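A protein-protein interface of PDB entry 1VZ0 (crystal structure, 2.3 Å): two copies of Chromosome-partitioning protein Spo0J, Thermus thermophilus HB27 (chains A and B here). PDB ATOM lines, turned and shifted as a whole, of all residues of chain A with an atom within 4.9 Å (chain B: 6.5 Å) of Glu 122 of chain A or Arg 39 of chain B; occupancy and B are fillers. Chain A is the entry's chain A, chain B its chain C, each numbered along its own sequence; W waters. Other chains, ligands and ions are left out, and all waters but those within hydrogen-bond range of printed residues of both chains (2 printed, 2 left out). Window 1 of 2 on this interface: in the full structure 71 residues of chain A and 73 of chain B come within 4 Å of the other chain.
Asp 117 of chain B touches its own counterpart, Asp 117 of chain A. Positions printed for both chains: 115 and 117.
Water W2 lies within hydrogen-bond range of ND2 of Asn 112 of chain A (2.8 Å) and N of Arg 39 of chain B (3.0 Å). Water W1 lies within hydrogen-bond range of O of Arg 39 of chain B (2.8 Å), OE1 of Glu 122 of chain A (3.0 Å) and N of Ala 43 of chain B (3.5 Å).
Among the printed residues, pairs that only touch across the chains: Leu 118 of chain A with Arg 39 of chain B (3.3 Å), Arg 125 of chain A with Phe 42 of chain B (3.4 Å), Glu 169 of chain A with Arg 115 of chain B (3.5 Å), Asn 112 of chain A with Arg 39 of chain B (3.6 Å), Ser 119 of chain A with Glu 116 of chain B (3.6 Å), Ser 119 of chain A with Asp 117 of chain B (3.7 Å), Pro 120 of chain A with Glu 116 of chain B (3.8 Å) and Gly 126 of chain A with Phe 42 of chain B (3.9 Å).
OG of Ser 119 of chain A lies close to N of Val 121 of chain A, at 3.2 Å. The guanidinium group (NH1) of Arg 115 of chain B is in salt-bridge range of the side-chain carboxylate (OD1) of Asp 117 of chain B, at 2.9 Å. NH1 of Arg 115 of chain A is in salt-bridge range of OD1 of Asp 117 of chain A (2.9 Å). OG of Ser 119 of chain A sits at hydrogen-bond distance from N of Glu 122 of chain A. OG of Ser 119 of chain A sits at hydrogen-bond distance from OE1 of Glu 169 of chain A (2.6 Å).
Of the 14 printed residues of chain A, 10 touch a printed residue of chain B. Hydrophobic or aromatic side chains of chain B within 4 Å of the printed part of chain A: Phe 42. Among the printed residues, 15 pairs touch across the chains. Among the printed residues, Asp or Glu carboxylates within 4 Å of a Lys or Arg side-chain nitrogen of the other chain: Asp 117 of chain A with Arg 39 of chain B and Glu 122 of chain A with Arg 39 of chain B.
O of Asp 117 of chain A sits close to O of Asp 117 of chain B (3.2 Å). The guanidinium group (NE) of Arg 115 of chain A lies close to the guanidinium group (NH2) of Arg 39 of chain B (3.1 Å). OD2 of Asp 117 of chain B lies close to OE2 of Glu 122 of chain A. The backbone carbonyl oxygen (O) of Glu 169 of chain A sits at hydrogen-bond distance from the backbone NH (N) of Glu 116 of chain B (3.2 Å). OD1 of Asp 117 of chain A is in salt-bridge range of NH2 of Arg 39 of chain B (3.3 Å). The backbone carbonyl oxygen of Glu 116 of chain B lies close to the backbone carbonyl oxygen of Leu 118 of chain A, 3.5 Å away. NH1 of Arg 39 of chain B lies within salt-bridge range of OE1 of Glu 122 of chain A (2.8 Å).
Of chain B, only Arg 39 and Asp 117 come within 4 Å of Glu 122 of chain A. Of chain A, only Asn 112 (3.6 Å), Arg 115 (3.1 Å), Asp 117 (3.0 Å), Leu 118 (3.3 Å) and Glu 122 (2.8 Å) come within 4 Å of Arg 39 of chain B. Of the printed residues of chain B, Asn 112 of chain A touches Arg 39. Printed residues of chain B within 4 Å of Leu 118 of chain A: Arg 39 and Glu 116. Printed residues of chain A within 4 Å of Glu 116 of chain B: Leu 118 (3.5 Å), Ser 119 (3.6 Å), Pro 120 (3.8 Å) and Glu 169 (3.2 Å). Of the printed residues of chain B, Glu 169 of chain A touches Arg 115 and Glu 116. The nearest residue of chain B that does not touch Glu 122 of chain A is Phe 42 of chain B (4.6 Å). The nearest printed residue of chain B that does not touch Asn 112 of chain A is Pro 38 of chain B (4.3 Å).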
ATOM      1  N   ASN A 112      -6.909  -9.830   5.818  1.00  0.00           N
ATOM      2  CA  ASN A 112      -6.814  -9.704   7.263  1.00  0.00           C
ATOM      3  C   ASN A 112      -5.506 -10.359   7.732  1.00  0.00           C
ATOM      4  O   ASN A 112      -4.803  -9.830   8.597  1.00  0.00           O
ATOM      5  CB  ASN A 112      -8.025 -10.382   7.903  1.00  0.00           C
ATOM      6  CG  ASN A 112      -8.343  -9.836   9.274  1.00  0.00           C
ATOM      7  OD1 ASN A 112      -7.699 -10.189  10.259  1.00  0.00           O
ATOM      8  ND2 ASN A 112      -9.347  -8.959   9.347  1.00  0.00           N
ATOM      9  N   LEU A 113      -5.176 -11.506   7.141  1.00  0.00           N
ATOM     10  CA  LEU A 113      -3.960 -12.235   7.497  1.00  0.00           C
ATOM     11  C   LEU A 113      -2.671 -11.529   7.081  1.00  0.00           C
ATOM     12  O   LEU A 113      -1.594 -11.910   7.532  1.00  0.00           O
ATOM     13  CB  LEU A 113      -3.986 -13.639   6.880  1.00  0.00           C
ATOM     14  CG  LEU A 113      -4.962 -14.610   7.535  1.00  0.00           C
ATOM     15  CD1 LEU A 113      -5.218 -15.790   6.616  1.00  0.00           C
ATOM     16  CD2 LEU A 113      -4.387 -15.053   8.882  1.00  0.00           C
ATOM     17  N   ARG A 115      -2.250  -8.199   7.523  1.00  0.00           N
ATOM     18  CA  ARG A 115      -2.092  -7.074   8.457  1.00  0.00           C
ATOM     19  C   ARG A 115      -0.987  -7.213   9.523  1.00  0.00           C
ATOM     20  O   ARG A 115      -0.627  -8.325   9.919  1.00  0.00           O
ATOM     21  CB  ARG A 115      -3.425  -6.801   9.168  1.00  0.00           C
ATOM     22  CG  ARG A 115      -4.573  -6.417   8.254  1.00  0.00           C
ATOM     23  CD  ARG A 115      -5.831  -6.129   9.070  1.00  0.00           C
ATOM     24  NE  ARG A 115      -5.642  -5.015   9.993  1.00  0.00           N
ATOM     25  CZ  ARG A 115      -5.659  -3.729   9.647  1.00  0.00           C
ATOM     26  NH1 ARG A 115      -5.466  -2.792  10.568  1.00  0.00           N
ATOM     27  NH2 ARG A 115      -5.891  -3.379   8.388  1.00  0.00           N
ATOM     28  N   ASP A 117      -1.425  -6.298  12.306  1.00  0.00           N
ATOM     29  CA  ASP A 117      -2.357  -6.326  13.427  1.00  0.00           C
ATOM     30  C   ASP A 117      -2.663  -7.644  14.123  1.00  0.00           C
ATOM     31  O   ASP A 117      -3.385  -7.660  15.118  1.00  0.00           O
ATOM     32  CB  ASP A 117      -3.690  -5.802  12.915  1.00  0.00           C
ATOM     33  CG  ASP A 117      -4.059  -4.530  13.538  1.00  0.00           C
ATOM     34  OD1 ASP A 117      -5.127  -3.992  13.179  1.00  0.00           O
ATOM     35  OD2 ASP A 117      -3.265  -4.080  14.393  1.00  0.00           O
ATOM     36  N   LEU A 118      -2.157  -8.745  13.603  1.00  0.00           N
ATOM     37  CA  LEU A 118      -2.513 -10.026  14.175  1.00  0.00           C
ATOM     38  C   LEU A 118      -1.662 -10.680  15.224  1.00  0.00           C
ATOM     39  O   LEU A 118      -0.438 -10.626  15.200  1.00  0.00           O
ATOM     40  CB  LEU A 118      -2.728 -11.042  13.057  1.00  0.00           C
ATOM     41  CG  LEU A 118      -4.141 -11.119  12.498  1.00  0.00           C
ATOM     42  CD1 LEU A 118      -4.547  -9.781  11.876  1.00  0.00           C
ATOM     43  CD2 LEU A 118      -4.187 -12.248  11.483  1.00  0.00           C
ATOM     44  N   SER A 119      -2.354 -11.340  16.137  1.00  0.00           N
ATOM     45  CA  SER A 119      -1.713 -12.102  17.180  1.00  0.00           C
ATOM     46  C   SER A 119      -1.580 -13.469  16.518  1.00  0.00           C
ATOM     47  O   SER A 119      -2.300 -13.769  15.558  1.00  0.00           O
ATOM     48  CB  SER A 119      -2.633 -12.222  18.386  1.00  0.00           C
ATOM     49  OG  SER A 119      -3.655 -13.180  18.141  1.00  0.00           O
ATOM     50  N   PRO A 120      -0.654 -14.309  16.998  1.00  0.00           N
ATOM     51  CA  PRO A 120      -0.521 -15.629  16.372  1.00  0.00           C
ATOM     52  C   PRO A 120      -1.784 -16.496  16.489  1.00  0.00           C
ATOM     53  O   PRO A 120      -1.960 -17.443  15.732  1.00  0.00           O
ATOM     54  CB  PRO A 120       0.710 -16.235  17.065  1.00  0.00           C
ATOM     55  CG  PRO A 120       0.884 -15.418  18.322  1.00  0.00           C
ATOM     56  CD  PRO A 120       0.472 -14.030  17.906  1.00  0.00           C
ATOM     57  N   VAL A 121      -2.665 -16.169  17.427  1.00  0.00           N
ATOM     58  CA  VAL A 121      -3.906 -16.920  17.585  1.00  0.00           C
ATOM     59  C   VAL A 121      -4.890 -16.555  16.461  1.00  0.00           C
ATOM     60  O   VAL A 121      -5.558 -17.433  15.898  1.00  0.00           O
ATOM     61  CB  VAL A 121      -4.565 -16.628  18.947  1.00  0.00           C
ATOM     62  CG1 VAL A 121      -5.906 -17.349  19.055  1.00  0.00           C
ATOM     63  CG2 VAL A 121      -3.635 -17.059  20.067  1.00  0.00           C
ATOM     64  N   GLU A 122      -4.984 -15.263  16.138  1.00  0.00           N
ATOM     65  CA  GLU A 122      -5.884 -14.829  15.066  1.00  0.00           C
ATOM     66  C   GLU A 122      -5.399 -15.404  13.752  1.00  0.00           C
ATOM     67  O   GLU A 122      -6.192 -15.811  12.911  1.00  0.00           O
ATOM     68  CB  GLU A 122      -5.925 -13.309  14.964  1.00  0.00           C
ATOM     69  CG  GLU A 122      -6.468 -12.620  16.202  1.00  0.00           C
ATOM     70  CD  GLU A 122      -6.404 -11.112  16.078  1.00  0.00           C
ATOM     71  OE1 GLU A 122      -7.309 -10.517  15.455  1.00  0.00           O
ATOM     72  OE2 GLU A 122      -5.431 -10.527  16.595  1.00  0.00           O
ATOM     73  N   GLU A 123      -4.083 -15.422  13.587  1.00  0.00           N
ATOM     74  CA  GLU A 123      -3.456 -15.963  12.400  1.00  0.00           C
ATOM     75  C   GLU A 123      -3.910 -17.425  12.237  1.00  0.00           C
ATOM     76  O   GLU A 123      -4.270 -17.851  11.144  1.00  0.00           O
ATOM     77  CB  GLU A 123      -1.937 -15.861  12.564  1.00  0.00           C
ATOM     78  CG  GLU A 123      -1.110 -16.616  11.554  1.00  0.00           C
ATOM     79  CD  GLU A 123       0.382 -16.521  11.848  1.00  0.00           C
ATOM     80  OE1 GLU A 123       1.179 -17.226  11.182  1.00  0.00           O
ATOM     81  OE2 GLU A 123       0.753 -15.731  12.746  1.00  0.00           O
ATOM     82  N   ALA A 124      -3.913 -18.176  13.333  1.00  0.00           N
ATOM     83  CA  ALA A 124      -4.336 -19.569  13.306  1.00  0.00           C
ATOM     84  C   ALA A 124      -5.807 -19.683  12.944  1.00  0.00           C
ATOM     85  O   ALA A 124      -6.186 -20.552  12.159  1.00  0.00           O
ATOM     86  CB  ALA A 124      -4.095 -20.231  14.664  1.00  0.00           C
ATOM     87  N   ARG A 125      -6.636 -18.821  13.532  1.00  0.00           N
ATOM     88  CA  ARG A 125      -8.068 -18.852  13.259  1.00  0.00           C
ATOM     89  C   ARG A 125      -8.338 -18.539  11.794  1.00  0.00           C
ATOM     90  O   ARG A 125      -9.259 -19.095  11.192  1.00  0.00           O
ATOM     91  CB  ARG A 125      -8.825 -17.853  14.149  1.00  0.00           C
ATOM     92  CG  ARG A 125      -8.739 -18.146  15.639  1.00  0.00           C
ATOM     93  CD  ARG A 125      -9.668 -17.243  16.444  1.00  0.00           C
ATOM     94  NE  ARG A 125      -9.411 -17.373  17.873  1.00  0.00           N
ATOM     95  CZ  ARG A 125      -9.830 -18.390  18.621  1.00  0.00           C
ATOM     96  NH1 ARG A 125      -9.535 -18.429  19.916  1.00  0.00           N
ATOM     97  NH2 ARG A 125     -10.564 -19.358  18.080  1.00  0.00           N
ATOM     98  N   GLY A 126      -7.539 -17.640  11.228  1.00  0.00           N
ATOM     99  CA  GLY A 126      -7.709 -17.293   9.830  1.00  0.00           C
ATOM    100  C   GLY A 126      -7.394 -18.492   8.946  1.00  0.00           C
ATOM    101  O   GLY A 126      -8.155 -18.823   8.028  1.00  0.00           O
ATOM    102  N   GLU A 169      -2.490 -13.909  23.854  1.00  0.00           N
ATOM    103  CA  GLU A 169      -2.931 -12.670  23.230  1.00  0.00           C
ATOM    104  C   GLU A 169      -2.625 -11.444  24.085  1.00  0.00           C
ATOM    105  O   GLU A 169      -2.364 -10.371  23.546  1.00  0.00           O
ATOM    106  CB  GLU A 169      -4.432 -12.727  22.920  1.00  0.00           C
ATOM    107  CG  GLU A 169      -4.825 -13.918  22.053  1.00  0.00           C
ATOM    108  CD  GLU A 169      -5.813 -13.555  20.965  1.00  0.00           C
ATOM    109  OE1 GLU A 169      -5.418 -12.834  20.025  1.00  0.00           O
ATOM    110  OE2 GLU A 169      -6.981 -13.988  21.047  1.00  0.00           O
ATOM    111  N   ARG B  36     -18.452  -9.040   5.336  1.00  0.00           N
ATOM    112  CA  ARG B  36     -17.483 -10.009   5.850  1.00  0.00           C
ATOM    113  C   ARG B  36     -16.550  -9.325   6.844  1.00  0.00           C
ATOM    114  O   ARG B  36     -15.736  -8.480   6.471  1.00  0.00           O
ATOM    115  CB  ARG B  36     -16.658 -10.598   4.710  1.00  0.00           C
ATOM    116  CG  ARG B  36     -17.492 -11.292   3.667  1.00  0.00           C
ATOM    117  CD  ARG B  36     -16.804 -11.275   2.314  1.00  0.00           C
ATOM    118  NE  ARG B  36     -17.804 -11.199   1.268  1.00  0.00           N
ATOM    119  CZ  ARG B  36     -18.280 -10.074   0.741  1.00  0.00           C
ATOM    120  NH1 ARG B  36     -19.206 -10.146  -0.197  1.00  0.00           N
ATOM    121  NH2 ARG B  36     -17.810  -8.887   1.102  1.00  0.00           N
ATOM    122  N   GLN B  37     -16.674  -9.693   8.110  1.00  0.00           N
ATOM    123  CA  GLN B  37     -15.848  -9.098   9.152  1.00  0.00           C
ATOM    124  C   GLN B  37     -15.258 -10.221   9.998  1.00  0.00           C
ATOM    125  O   GLN B  37     -15.547 -10.335  11.186  1.00  0.00           O
ATOM    126  CB  GLN B  37     -16.704  -8.165  10.019  1.00  0.00           C
ATOM    127  CG  GLN B  37     -17.351  -6.998   9.266  1.00  0.00           C
ATOM    128  CD  GLN B  37     -16.348  -5.930   8.846  1.00  0.00           C
ATOM    129  OE1 GLN B  37     -15.439  -5.583   9.601  1.00  0.00           O
ATOM    130  NE2 GLN B  37     -16.525  -5.389   7.645  1.00  0.00           N
ATOM    131  N   PRO B  38     -14.419 -11.068   9.387  1.00  0.00           N
ATOM    132  CA  PRO B  38     -13.787 -12.194  10.085  1.00  0.00           C
ATOM    133  C   PRO B  38     -13.099 -11.838  11.410  1.00  0.00           C
ATOM    134  O   PRO B  38     -13.176 -12.601  12.376  1.00  0.00           O
ATOM    135  CB  PRO B  38     -12.818 -12.751   9.038  1.00  0.00           C
ATOM    136  CG  PRO B  38     -12.518 -11.568   8.169  1.00  0.00           C
ATOM    137  CD  PRO B  38     -13.867 -10.919   8.029  1.00  0.00           C
ATOM    138  N   ARG B  39     -12.441 -10.688  11.463  1.00  0.00           N
ATOM    139  CA  ARG B  39     -11.772 -10.261  12.690  1.00  0.00           C
ATOM    140  C   ARG B  39     -12.775 -10.152  13.844  1.00  0.00           C
ATOM    141  O   ARG B  39     -12.532 -10.639  14.953  1.00  0.00           O
ATOM    142  CB  ARG B  39     -11.099  -8.909  12.479  1.00  0.00           C
ATOM    143  CG  ARG B  39     -10.669  -8.240  13.770  1.00  0.00           C
ATOM    144  CD  ARG B  39      -9.200  -8.452  14.050  1.00  0.00           C
ATOM    145  NE  ARG B  39      -8.378  -7.689  13.119  1.00  0.00           N
ATOM    146  CZ  ARG B  39      -7.055  -7.593  13.192  1.00  0.00           C
ATOM    147  NH1 ARG B  39      -6.390  -8.214  14.159  1.00  0.00           N
ATOM    148  NH2 ARG B  39      -6.397  -6.870  12.297  1.00  0.00           N
ATOM    149  N   LYS B  40     -13.906  -9.512  13.579  1.00  0.00           N
ATOM    150  CA  LYS B  40     -14.921  -9.354  14.604  1.00  0.00           C
ATOM    151  C   LYS B  40     -15.545 -10.693  14.948  1.00  0.00           C
ATOM    152  O   LYS B  40     -15.845 -10.971  16.112  1.00  0.00           O
ATOM    153  CB  LYS B  40     -16.001  -8.375  14.137  1.00  0.00           C
ATOM    154  CG  LYS B  40     -15.498  -6.946  13.960  1.00  0.00           C
ATOM    155  CD  LYS B  40     -16.630  -6.011  13.549  1.00  0.00           C
ATOM    156  CE  LYS B  40     -16.121  -4.620  13.194  1.00  0.00           C
ATOM    157  NZ  LYS B  40     -15.465  -3.950  14.345  1.00  0.00           N
ATOM    158  N   ARG B  41     -15.726 -11.529  13.935  1.00  0.00           N
ATOM    159  CA  ARG B  41     -16.330 -12.836  14.143  1.00  0.00           C
ATOM    160  C   ARG B  41     -15.446 -13.699  15.025  1.00  0.00           C
ATOM    161  O   ARG B  41     -15.937 -14.414  15.902  1.00  0.00           O
ATOM    162  CB  ARG B  41     -16.581 -13.517  12.793  1.00  0.00           C
ATOM    163  CG  ARG B  41     -17.987 -14.057  12.649  1.00  0.00           C
ATOM    164  CD  ARG B  41     -19.023 -13.001  13.065  1.00  0.00           C
ATOM    165  NE  ARG B  41     -18.999 -11.815  12.212  1.00  0.00           N
ATOM    166  CZ  ARG B  41     -19.481 -10.621  12.551  1.00  0.00           C
ATOM    167  NH1 ARG B  41     -19.410  -9.619  11.689  1.00  0.00           N
ATOM    168  NH2 ARG B  41     -20.012 -10.418  13.748  1.00  0.00           N
ATOM    169  N   PHE B  42     -14.139 -13.621  14.792  1.00  0.00           N
ATOM    170  CA  PHE B  42     -13.166 -14.379  15.568  1.00  0.00           C
ATOM    171  C   PHE B  42     -13.134 -13.920  17.021  1.00  0.00           C
ATOM    172  O   PHE B  42     -13.024 -14.735  17.936  1.00  0.00           O
ATOM    173  CB  PHE B  42     -11.783 -14.226  14.945  1.00  0.00           C
ATOM    174  CG  PHE B  42     -11.623 -14.961  13.645  1.00  0.00           C
ATOM    175  CD1 PHE B  42     -10.729 -14.511  12.683  1.00  0.00           C
ATOM    176  CD2 PHE B  42     -12.349 -16.123  13.393  1.00  0.00           C
ATOM    177  CE1 PHE B  42     -10.559 -15.209  11.492  1.00  0.00           C
ATOM    178  CE2 PHE B  42     -12.186 -16.828  12.206  1.00  0.00           C
ATOM    179  CZ  PHE B  42     -11.287 -16.370  11.253  1.00  0.00           C
ATOM    180  N   ALA B  43     -13.232 -12.613  17.235  1.00  0.00           N
ATOM    181  CA  ALA B  43     -13.222 -12.079  18.591  1.00  0.00           C
ATOM    182  C   ALA B  43     -14.435 -12.594  19.372  1.00  0.00           C
ATOM    183  O   ALA B  43     -14.313 -12.968  20.532  1.00  0.00           O
ATOM    184  CB  ALA B  43     -13.217 -10.549  18.554  1.00  0.00           C
ATOM    185  N   GLU B  44     -15.598 -12.628  18.724  1.00  0.00           N
ATOM    186  CA  GLU B  44     -16.825 -13.104  19.364  1.00  0.00           C
ATOM    187  C   GLU B  44     -16.741 -14.592  19.673  1.00  0.00           C
ATOM    188  O   GLU B  44     -17.167 -15.033  20.740  1.00  0.00           O
ATOM    189  CB  GLU B  44     -18.044 -12.859  18.467  1.00  0.00           C
ATOM    190  CG  GLU B  44     -18.179 -11.426  17.980  1.00  0.00           C
ATOM    191  CD  GLU B  44     -19.412 -11.198  17.123  1.00  0.00           C
ATOM    192  OE1 GLU B  44     -19.704 -12.035  16.239  1.00  0.00           O
ATOM    193  OE2 GLU B  44     -20.082 -10.164  17.325  1.00  0.00           O
ATOM    194  N   ARG B 115       0.299  -6.543  24.403  1.00  0.00           N
ATOM    195  CA  ARG B 115      -0.415  -7.519  23.586  1.00  0.00           C
ATOM    196  C   ARG B 115       0.320  -7.924  22.315  1.00  0.00           C
ATOM    197  O   ARG B 115       1.075  -7.146  21.742  1.00  0.00           O
ATOM    198  CB  ARG B 115      -1.794  -6.980  23.209  1.00  0.00           C
ATOM    199  CG  ARG B 115      -2.660  -6.604  24.387  1.00  0.00           C
ATOM    200  CD  ARG B 115      -3.985  -6.049  23.915  1.00  0.00           C
ATOM    201  NE  ARG B 115      -4.656  -7.004  23.040  1.00  0.00           N
ATOM    202  CZ  ARG B 115      -5.273  -8.112  23.450  1.00  0.00           C
ATOM    203  NH1 ARG B 115      -5.842  -8.916  22.563  1.00  0.00           N
ATOM    204  NH2 ARG B 115      -5.348  -8.409  24.740  1.00  0.00           N
ATOM    205  N   GLU B 116       0.091  -9.162  21.890  1.00  0.00           N
ATOM    206  CA  GLU B 116       0.690  -9.703  20.677  1.00  0.00           C
ATOM    207  C   GLU B 116      -0.028  -9.078  19.482  1.00  0.00           C
ATOM    208  O   GLU B 116       0.309  -9.321  18.325  1.00  0.00           O
ATOM    209  CB  GLU B 116       0.516 -11.221  20.655  1.00  0.00           C
ATOM    210  CG  GLU B 116       1.533 -11.974  21.476  1.00  0.00           C
ATOM    211  CD  GLU B 116       2.861 -12.097  20.757  1.00  0.00           C
ATOM    212  OE1 GLU B 116       3.507 -11.056  20.504  1.00  0.00           O
ATOM    213  OE2 GLU B 116       3.252 -13.236  20.433  1.00  0.00           O
ATOM    214  N   ASP B 117      -1.019  -8.262  19.815  1.00  0.00           N
ATOM    215  CA  ASP B 117      -1.880  -7.540  18.888  1.00  0.00           C
ATOM    216  C   ASP B 117      -1.283  -6.288  18.249  1.00  0.00           C
ATOM    217  O   ASP B 117      -1.702  -5.885  17.177  1.00  0.00           O
ATOM    218  CB  ASP B 117      -3.143  -7.107  19.640  1.00  0.00           C
ATOM    219  CG  ASP B 117      -4.313  -7.963  19.326  1.00  0.00           C
ATOM    220  OD1 ASP B 117      -5.369  -7.765  19.947  1.00  0.00           O
ATOM    221  OD2 ASP B 117      -4.175  -8.832  18.444  1.00  0.00           O
HETATM  222  O   HOH W   1     -10.133 -11.323  16.267  1.00  0.00           O
HETATM  223  O   HOH W   2     -12.098  -8.373   9.535  1.00  0.00           O
